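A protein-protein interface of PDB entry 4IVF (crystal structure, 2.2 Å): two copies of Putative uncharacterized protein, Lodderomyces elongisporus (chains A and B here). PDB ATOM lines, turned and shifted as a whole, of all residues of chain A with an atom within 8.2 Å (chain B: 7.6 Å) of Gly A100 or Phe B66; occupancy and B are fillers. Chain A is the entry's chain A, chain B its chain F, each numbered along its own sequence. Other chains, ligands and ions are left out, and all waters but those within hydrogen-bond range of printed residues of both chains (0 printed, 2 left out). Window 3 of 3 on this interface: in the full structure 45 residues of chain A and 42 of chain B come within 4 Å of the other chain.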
ATOM      1  N   TYR A  97     -27.218 -37.383   6.488  1.00  0.00           N
ATOM      2  CA  TYR A  97     -26.128 -36.657   5.860  1.00  0.00           C
ATOM      3  C   TYR A  97     -24.816 -36.957   6.560  1.00  0.00           C
ATOM      4  O   TYR A  97     -24.820 -37.355   7.717  1.00  0.00           O
ATOM      5  CB  TYR A  97     -26.420 -35.160   5.887  1.00  0.00           C
ATOM      6  CG  TYR A  97     -27.557 -34.790   4.966  1.00  0.00           C
ATOM      7  CD1 TYR A  97     -27.319 -34.446   3.630  1.00  0.00           C
ATOM      8  CD2 TYR A  97     -28.871 -34.804   5.421  1.00  0.00           C
ATOM      9  CE1 TYR A  97     -28.370 -34.108   2.782  1.00  0.00           C
ATOM     10  CE2 TYR A  97     -29.917 -34.477   4.587  1.00  0.00           C
ATOM     11  CZ  TYR A  97     -29.664 -34.129   3.274  1.00  0.00           C
ATOM     12  OH  TYR A  97     -30.715 -33.813   2.463  1.00  0.00           O
ATOM     13  N   PRO A  98     -23.686 -36.772   5.849  1.00  0.00           N
ATOM     14  CA  PRO A  98     -22.370 -37.022   6.445  1.00  0.00           C
ATOM     15  C   PRO A  98     -22.167 -36.192   7.710  1.00  0.00           C
ATOM     16  O   PRO A  98     -22.605 -35.045   7.759  1.00  0.00           O
ATOM     17  CB  PRO A  98     -21.398 -36.591   5.344  1.00  0.00           C
ATOM     18  CG  PRO A  98     -22.169 -36.761   4.095  1.00  0.00           C
ATOM     19  CD  PRO A  98     -23.581 -36.387   4.430  1.00  0.00           C
ATOM     20  N   ALA A  99     -21.525 -36.783   8.714  1.00  0.00           N
ATOM     21  CA  ALA A  99     -21.326 -36.128  10.002  1.00  0.00           C
ATOM     22  C   ALA A  99     -20.625 -34.789   9.853  1.00  0.00           C
ATOM     23  O   ALA A  99     -19.728 -34.640   9.032  1.00  0.00           O
ATOM     24  CB  ALA A  99     -20.538 -37.031  10.947  1.00  0.00           C
ATOM     25  N   GLY A 100     -21.047 -33.810  10.647  1.00  0.00           N
ATOM     26  CA  GLY A 100     -20.368 -32.530  10.668  1.00  0.00           C
ATOM     27  C   GLY A 100     -20.695 -31.611   9.504  1.00  0.00           C
ATOM     28  O   GLY A 100     -20.116 -30.531   9.397  1.00  0.00           O
ATOM     29  N   THR A 101     -21.603 -32.029   8.625  1.00  0.00           N
ATOM     30  CA  THR A 101     -22.103 -31.120   7.592  1.00  0.00           C
ATOM     31  C   THR A 101     -23.270 -30.276   8.114  1.00  0.00           C
ATOM     32  O   THR A 101     -23.907 -30.627   9.099  1.00  0.00           O
ATOM     33  CB  THR A 101     -22.559 -31.857   6.317  1.00  0.00           C
ATOM     34  OG1 THR A 101     -23.646 -32.737   6.627  1.00  0.00           O
ATOM     35  CG2 THR A 101     -21.403 -32.644   5.693  1.00  0.00           C
ATOM     36  N   ALA A 102     -23.533 -29.165   7.434  1.00  0.00           N
ATOM     37  CA  ALA A 102     -24.639 -28.287   7.768  1.00  0.00           C
ATOM     38  C   ALA A 102     -25.949 -29.051   7.745  1.00  0.00           C
ATOM     39  O   ALA A 102     -26.754 -28.917   8.662  1.00  0.00           O
ATOM     40  CB  ALA A 102     -24.702 -27.118   6.801  1.00  0.00           C
ATOM     41  N   GLU A 103     -26.157 -29.844   6.695  1.00  0.00           N
ATOM     42  CA  GLU A 103     -27.384 -30.620   6.562  1.00  0.00           C
ATOM     43  C   GLU A 103     -27.527 -31.639   7.700  1.00  0.00           C
ATOM     44  O   GLU A 103     -28.636 -31.959   8.133  1.00  0.00           O
ATOM     45  CB  GLU A 103     -27.465 -31.309   5.195  1.00  0.00           C
ATOM     46  CG  GLU A 103     -27.636 -30.368   4.004  1.00  0.00           C
ATOM     47  CD  GLU A 103     -26.311 -29.812   3.488  1.00  0.00           C
ATOM     48  OE1 GLU A 103     -25.243 -30.253   3.968  1.00  0.00           O
ATOM     49  OE2 GLU A 103     -26.336 -28.930   2.600  1.00  0.00           O
ATOM     50  N   TYR A 104     -26.401 -32.149   8.186  1.00  0.00           N
ATOM     51  CA  TYR A 104     -26.433 -33.052   9.332  1.00  0.00           C
ATOM     52  C   TYR A 104     -26.944 -32.326  10.583  1.00  0.00           C
ATOM     53  O   TYR A 104     -27.814 -32.833  11.294  1.00  0.00           O
ATOM     54  CB  TYR A 104     -25.057 -33.657   9.576  1.00  0.00           C
ATOM     55  CG  TYR A 104     -24.905 -34.398  10.893  1.00  0.00           C
ATOM     56  CD1 TYR A 104     -25.250 -35.742  11.008  1.00  0.00           C
ATOM     57  CD2 TYR A 104     -24.379 -33.759  12.014  1.00  0.00           C
ATOM     58  CE1 TYR A 104     -25.088 -36.429  12.216  1.00  0.00           C
ATOM     59  CE2 TYR A 104     -24.212 -34.432  13.221  1.00  0.00           C
ATOM     60  CZ  TYR A 104     -24.564 -35.762  13.316  1.00  0.00           C
ATOM     61  OH  TYR A 104     -24.392 -36.414  14.517  1.00  0.00           O
ATOM     62  N   TYR A 105     -26.411 -31.134  10.838  1.00  0.00           N
ATOM     63  CA  TYR A 105     -26.828 -30.360  11.995  1.00  0.00           C
ATOM     64  C   TYR A 105     -28.242 -29.789  11.877  1.00  0.00           C
ATOM     65  O   TYR A 105     -28.932 -29.639  12.892  1.00  0.00           O
ATOM     66  CB  TYR A 105     -25.800 -29.274  12.335  1.00  0.00           C
ATOM     67  CG  TYR A 105     -24.541 -29.865  12.904  1.00  0.00           C
ATOM     68  CD1 TYR A 105     -24.578 -30.596  14.080  1.00  0.00           C
ATOM     69  CD2 TYR A 105     -23.319 -29.724  12.251  1.00  0.00           C
ATOM     70  CE1 TYR A 105     -23.440 -31.176  14.598  1.00  0.00           C
ATOM     71  CE2 TYR A 105     -22.165 -30.291  12.766  1.00  0.00           C
ATOM     72  CZ  TYR A 105     -22.235 -31.022  13.943  1.00  0.00           C
ATOM     73  OH  TYR A 105     -21.102 -31.593  14.484  1.00  0.00           O
ATOM     74  N   LEU B   5     -10.031 -18.155  16.346  1.00  0.00           N
ATOM     75  CA  LEU B   5     -11.458 -18.253  16.027  1.00  0.00           C
ATOM     76  C   LEU B   5     -12.217 -16.928  16.109  1.00  0.00           C
ATOM     77  O   LEU B   5     -11.892 -16.058  16.919  1.00  0.00           O
ATOM     78  CB  LEU B   5     -12.156 -19.258  16.945  1.00  0.00           C
ATOM     79  CG  LEU B   5     -11.773 -20.736  16.849  1.00  0.00           C
ATOM     80  CD1 LEU B   5     -12.536 -21.557  17.889  1.00  0.00           C
ATOM     81  CD2 LEU B   5     -12.021 -21.269  15.450  1.00  0.00           C
ATOM     82  N   ASN B  62     -25.031 -18.301  15.862  1.00  0.00           N
ATOM     83  CA  ASN B  62     -24.436 -18.200  14.539  1.00  0.00           C
ATOM     84  C   ASN B  62     -22.942 -18.346  14.700  1.00  0.00           C
ATOM     85  O   ASN B  62     -22.287 -17.512  15.344  1.00  0.00           O
ATOM     86  CB  ASN B  62     -24.761 -16.870  13.838  1.00  0.00           C
ATOM     87  CG  ASN B  62     -24.223 -16.805  12.400  1.00  0.00           C
ATOM     88  OD1 ASN B  62     -23.204 -17.406  12.069  1.00  0.00           O
ATOM     89  ND2 ASN B  62     -24.911 -16.058  11.547  1.00  0.00           N
ATOM     90  N   ASP B  63     -22.416 -19.414  14.109  1.00  0.00           N
ATOM     91  CA  ASP B  63     -20.991 -19.679  14.129  1.00  0.00           C
ATOM     92  C   ASP B  63     -20.383 -19.273  12.805  1.00  0.00           C
ATOM     93  O   ASP B  63     -20.530 -19.981  11.811  1.00  0.00           O
ATOM     94  CB  ASP B  63     -20.718 -21.166  14.381  1.00  0.00           C
ATOM     95  CG  ASP B  63     -19.283 -21.426  14.803  1.00  0.00           C
ATOM     96  OD1 ASP B  63     -18.447 -20.515  14.627  1.00  0.00           O
ATOM     97  OD2 ASP B  63     -18.988 -22.531  15.306  1.00  0.00           O
ATOM     98  N   PRO B  64     -19.664 -18.144  12.789  1.00  0.00           N
ATOM     99  CA  PRO B  64     -19.014 -17.693  11.549  1.00  0.00           C
ATOM    100  C   PRO B  64     -17.805 -18.566  11.215  1.00  0.00           C
ATOM    101  O   PRO B  64     -17.233 -18.456  10.128  1.00  0.00           O
ATOM    102  CB  PRO B  64     -18.580 -16.261  11.880  1.00  0.00           C
ATOM    103  CG  PRO B  64     -18.392 -16.260  13.377  1.00  0.00           C
ATOM    104  CD  PRO B  64     -19.348 -17.289  13.948  1.00  0.00           C
ATOM    105  N   ASN B  65     -17.430 -19.435  12.151  1.00  0.00           N
ATOM    106  CA  ASN B  65     -16.303 -20.335  11.948  1.00  0.00           C
ATOM    107  C   ASN B  65     -16.667 -21.555  11.096  1.00  0.00           C
ATOM    108  O   ASN B  65     -15.786 -22.222  10.575  1.00  0.00           O
ATOM    109  CB  ASN B  65     -15.691 -20.767  13.291  1.00  0.00           C
ATOM    110  CG  ASN B  65     -15.111 -19.590  14.087  1.00  0.00           C
ATOM    111  OD1 ASN B  65     -14.121 -18.977  13.684  1.00  0.00           O
ATOM    112  ND2 ASN B  65     -15.723 -19.286  15.225  1.00  0.00           N
ATOM    113  N   PHE B  66     -17.960 -21.840  10.955  1.00  0.00           N
ATOM    114  CA  PHE B  66     -18.405 -22.946  10.103  1.00  0.00           C
ATOM    115  C   PHE B  66     -18.219 -22.585   8.632  1.00  0.00           C
ATOM    116  O   PHE B  66     -18.936 -21.740   8.101  1.00  0.00           O
ATOM    117  CB  PHE B  66     -19.868 -23.317  10.372  1.00  0.00           C
ATOM    118  CG  PHE B  66     -20.261 -24.675   9.831  1.00  0.00           C
ATOM    119  CD1 PHE B  66     -20.775 -24.809   8.552  1.00  0.00           C
ATOM    120  CD2 PHE B  66     -20.103 -25.818  10.605  1.00  0.00           C
ATOM    121  CE1 PHE B  66     -21.130 -26.053   8.049  1.00  0.00           C
ATOM    122  CE2 PHE B  66     -20.453 -27.067  10.111  1.00  0.00           C
ATOM    123  CZ  PHE B  66     -20.961 -27.185   8.824  1.00  0.00           C
ATOM    124  N   LYS B  67     -17.273 -23.244   7.973  1.00  0.00           N
ATOM    125  CA  LYS B  67     -16.854 -22.828   6.631  1.00  0.00           C
ATOM    126  C   LYS B  67     -17.773 -23.269   5.475  1.00  0.00           C
ATOM    127  O   LYS B  67     -17.763 -22.663   4.400  1.00  0.00           O
ATOM    128  CB  LYS B  67     -15.386 -23.211   6.375  1.00  0.00           C
ATOM    129  CG  LYS B  67     -15.083 -24.685   6.563  1.00  0.00           C
ATOM    130  CD  LYS B  67     -13.652 -24.928   7.045  1.00  0.00           C
ATOM    131  CE  LYS B  67     -13.559 -24.879   8.567  1.00  0.00           C
ATOM    132  NZ  LYS B  67     -12.457 -25.747   9.085  1.00  0.00           N
ATOM    133  N   GLY B  68     -18.574 -24.305   5.693  1.00  0.00           N
ATOM    134  CA  GLY B  68     -19.548 -24.712   4.695  1.00  0.00           C
ATOM    135  C   GLY B  68     -20.595 -23.660   4.322  1.00  0.00           C
ATOM    136  O   GLY B  68     -21.065 -23.630   3.187  1.00  0.00           O
ATOM    137  N   VAL B  69     -20.951 -22.791   5.267  1.00  0.00           N
ATOM    138  CA  VAL B  69     -22.093 -21.888   5.102  1.00  0.00           C
ATOM    139  C   VAL B  69     -21.716 -20.407   4.951  1.00  0.00           C
ATOM    140  O   VAL B  69     -20.948 -19.863   5.747  1.00  0.00           O
ATOM    141  CB  VAL B  69     -23.088 -22.026   6.294  1.00  0.00           C
ATOM    142  CG1 VAL B  69     -24.405 -21.316   5.988  1.00  0.00           C
ATOM    143  CG2 VAL B  69     -23.338 -23.489   6.618  1.00  0.00           C
ATOM    144  N   ASP B  70     -22.278 -19.762   3.930  1.00  0.00           N
ATOM    145  CA  ASP B  70     -22.135 -18.320   3.733  1.00  0.00           C
ATOM    146  C   ASP B  70     -22.820 -17.545   4.853  1.00  0.00           C
ATOM    147  O   ASP B  70     -24.033 -17.652   5.038  1.00  0.00           O
ATOM    148  CB  ASP B  70     -22.753 -17.906   2.398  1.00  0.00           C
ATOM    149  CG  ASP B  70     -21.732 -17.829   1.279  1.00  0.00           C
ATOM    150  OD1 ASP B  70     -20.721 -18.559   1.334  1.00  0.00           O
ATOM    151  OD2 ASP B  70     -21.946 -17.031   0.340  1.00  0.00           O
ATOM    152  N   GLY B  71     -22.047 -16.756   5.592  1.00  0.00           N
ATOM    153  CA  GLY B  71     -22.587 -16.012   6.717  1.00  0.00           C
ATOM    154  C   GLY B  71     -22.529 -16.812   8.008  1.00  0.00           C
ATOM    155  O   GLY B  71     -22.912 -16.330   9.071  1.00  0.00           O
ATOM    156  N   GLY B  72     -22.034 -18.041   7.913  1.00  0.00           N
ATOM    157  CA  GLY B  72     -21.873 -18.889   9.078  1.00  0.00           C
ATOM    158  C   GLY B  72     -23.063 -19.797   9.322  1.00  0.00           C
ATOM    159  O   GLY B  72     -24.138 -19.617   8.736  1.00  0.00           O
ATOM    160  N   LEU B  73     -22.874 -20.773  10.203  1.00  0.00           N
ATOM    161  CA  LEU B  73     -23.929 -21.717  10.520  1.00  0.00           C
ATOM    162  C   LEU B  73     -24.894 -21.142  11.550  1.00  0.00           C
ATOM    163  O   LEU B  73     -24.489 -20.679  12.611  1.00  0.00           O
ATOM    164  CB  LEU B  73     -23.333 -23.030  11.034  1.00  0.00           C
ATOM    165  CG  LEU B  73     -24.329 -24.151  11.313  1.00  0.00           C
ATOM    166  CD1 LEU B  73     -25.087 -24.500  10.043  1.00  0.00           C
ATOM    167  CD2 LEU B  73     -23.588 -25.378  11.883  1.00  0.00           C
ATOM    168  N   VAL B  74     -26.175 -21.169  11.219  1.00  0.00           N
ATOM    169  CA  VAL B  74     -27.206 -20.733  12.134  1.00  0.00           C
ATOM    170  C   VAL B  74     -27.898 -21.977  12.662  1.00  0.00           C
ATOM    171  O   VAL B  74     -28.354 -22.819  11.887  1.00  0.00           O
ATOM    172  CB  VAL B  74     -28.226 -19.820  11.438  1.00  0.00           C
ATOM    173  CG1 VAL B  74     -29.300 -19.399  12.415  1.00  0.00           C
ATOM    174  CG2 VAL B  74     -27.531 -18.596  10.849  1.00  0.00           C
ATOM    175  N   TYR B  84     -23.647 -29.811  18.693  1.00  0.00           N
ATOM    176  CA  TYR B  84     -22.787 -29.128  17.734  1.00  0.00           C
ATOM    177  C   TYR B  84     -21.493 -28.607  18.365  1.00  0.00           C
ATOM    178  O   TYR B  84     -20.412 -28.861  17.848  1.00  0.00           O
ATOM    179  CB  TYR B  84     -23.521 -27.969  17.028  1.00  0.00           C
ATOM    180  CG  TYR B  84     -22.553 -27.108  16.233  1.00  0.00           C
ATOM    181  CD1 TYR B  84     -22.047 -27.540  15.008  1.00  0.00           C
ATOM    182  CD2 TYR B  84     -22.103 -25.895  16.739  1.00  0.00           C
ATOM    183  CE1 TYR B  84     -21.124 -26.772  14.307  1.00  0.00           C
ATOM    184  CE2 TYR B  84     -21.187 -25.128  16.051  1.00  0.00           C
ATOM    185  CZ  TYR B  84     -20.706 -25.563  14.836  1.00  0.00           C
ATOM    186  OH  TYR B  84     -19.797 -24.776  14.163  1.00  0.00           O
ATOM    187  N   ASP B  87     -19.217 -31.565  19.467  1.00  0.00           N
ATOM    188  CA  ASP B  87     -18.582 -32.159  18.283  1.00  0.00           C
ATOM    189  C   ASP B  87     -17.443 -31.288  17.761  1.00  0.00           C
ATOM    190  O   ASP B  87     -16.370 -31.788  17.437  1.00  0.00           O
ATOM    191  CB  ASP B  87     -19.580 -32.325  17.129  1.00  0.00           C
ATOM    192  CG  ASP B  87     -20.622 -33.395  17.382  1.00  0.00           C
ATOM    193  OD1 ASP B  87     -20.467 -34.195  18.341  1.00  0.00           O
ATOM    194  OD2 ASP B  87     -21.600 -33.433  16.602  1.00  0.00           O
ATOM    195  N   THR B  88     -17.696 -29.982  17.681  1.00  0.00           N
ATOM    196  CA  THR B  88     -16.803 -29.062  16.996  1.00  0.00           C
ATOM    197  C   THR B  88     -15.642 -28.564  17.859  1.00  0.00           C
ATOM    198  O   THR B  88     -14.504 -28.472  17.390  1.00  0.00           O
ATOM    199  CB  THR B  88     -17.597 -27.845  16.437  1.00  0.00           C
ATOM    200  OG1 THR B  88     -18.681 -28.310  15.624  1.00  0.00           O
ATOM    201  CG2 THR B  88     -16.705 -26.939  15.607  1.00  0.00           C
ATOM    202  N   TYR B  89     -15.925 -28.254  19.121  1.00  0.00           N
ATOM    203  CA  TYR B  89     -14.955 -27.567  19.976  1.00  0.00           C
ATOM    204  C   TYR B  89     -14.443 -28.367  21.176  1.00  0.00           C
ATOM    205  O   TYR B  89     -13.686 -27.850  21.995  1.00  0.00           O
ATOM    206  CB  TYR B  89     -15.511 -26.200  20.413  1.00  0.00           C
ATOM    207  CG  TYR B  89     -15.812 -25.326  19.210  1.00  0.00           C
ATOM    208  CD1 TYR B  89     -14.772 -24.829  18.423  1.00  0.00           C
ATOM    209  CD2 TYR B  89     -17.126 -25.042  18.830  1.00  0.00           C
ATOM    210  CE1 TYR B  89     -15.025 -24.061  17.306  1.00  0.00           C
ATOM    211  CE2 TYR B  89     -17.394 -24.253  17.706  1.00  0.00           C
ATOM    212  CZ  TYR B  89     -16.330 -23.770  16.954  1.00  0.00           C
ATOM    213  OH  TYR B  89     -16.545 -23.008  15.845  1.00  0.00           O
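The side-chain hydroxyl (OH) of Tyr A105 is in hydrogen-bond range of the side-chain carboxylate (OD2) of Asp B87 (2.8 Å).
The side-chain hydroxyl of Tyr B84 lies within hydrogen-bond range of the side-chain carboxylate of Asp B63.
The side-chain hydroxyl (OG1) of Thr A101 is in hydrogen-bond range of the backbone NH (N) of Tyr A104.
The backbone carbonyl oxygen (O) of Tyr B84 lies within hydrogen-bond range of the side-chain hydroxyl (OG1) of Thr B88.
The backbone carbonyl oxygen of Pro A98 is in hydrogen-bond range of the side-chain hydroxyl of Thr A101 (2.8 Å).
Gly A100 touches Phe B66.
Phe B66 touches Thr A101 (CZ to C, 3.9 Å).
N of Ala A102 touches CZ of Phe B66, at 3.5 Å.
Val B69 touches Ala A102 (CG2 to CB, 3.9 Å).
Tyr A105 touches Tyr B84 (CE2 to CD1, 3.6 Å).
Gly A100 touches just one residue of chain B: Phe B66 (3.5 Å).
Of the printed residues of chain B, Ala A102 touches Phe B66 (3.5 Å) and Val B69 (3.9 Å).
Glu A103 touches none of the printed residues of chain B.
Of the printed residues of chain B, Tyr A105 touches Tyr B84 (3.6 Å) and Asp B87 (2.8 Å).
Phe B66 touches just these residues of chain A: Gly A100, Thr A101 and Ala A102.
Gly B72 touches none of the printed residues of chain A.
Printed residues of chain A within 4 Å of Asp B87: Tyr A105.
The nearest residue of chain A that does not touch Phe B66 is Tyr A105 (4.5 Å).
The nearest printed residue of chain B that does not touch Ala A102 is Leu B73 (4.2 Å).
Of the 9 printed residues of chain A, 4 touch a printed residue of chain B.
Along chain A the printed residues that touch a printed residue of chain B span positions 100 to 105.
Among the printed residues, no Asp or Glu carboxylate lies within 4 Å of a Lys or Arg side-chain nitrogen of the other chain.
No position is printed for both chains.
Of the 6 pairs that touch across the chains among the printed residues, none has its exchanged pair printed and touching as well.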
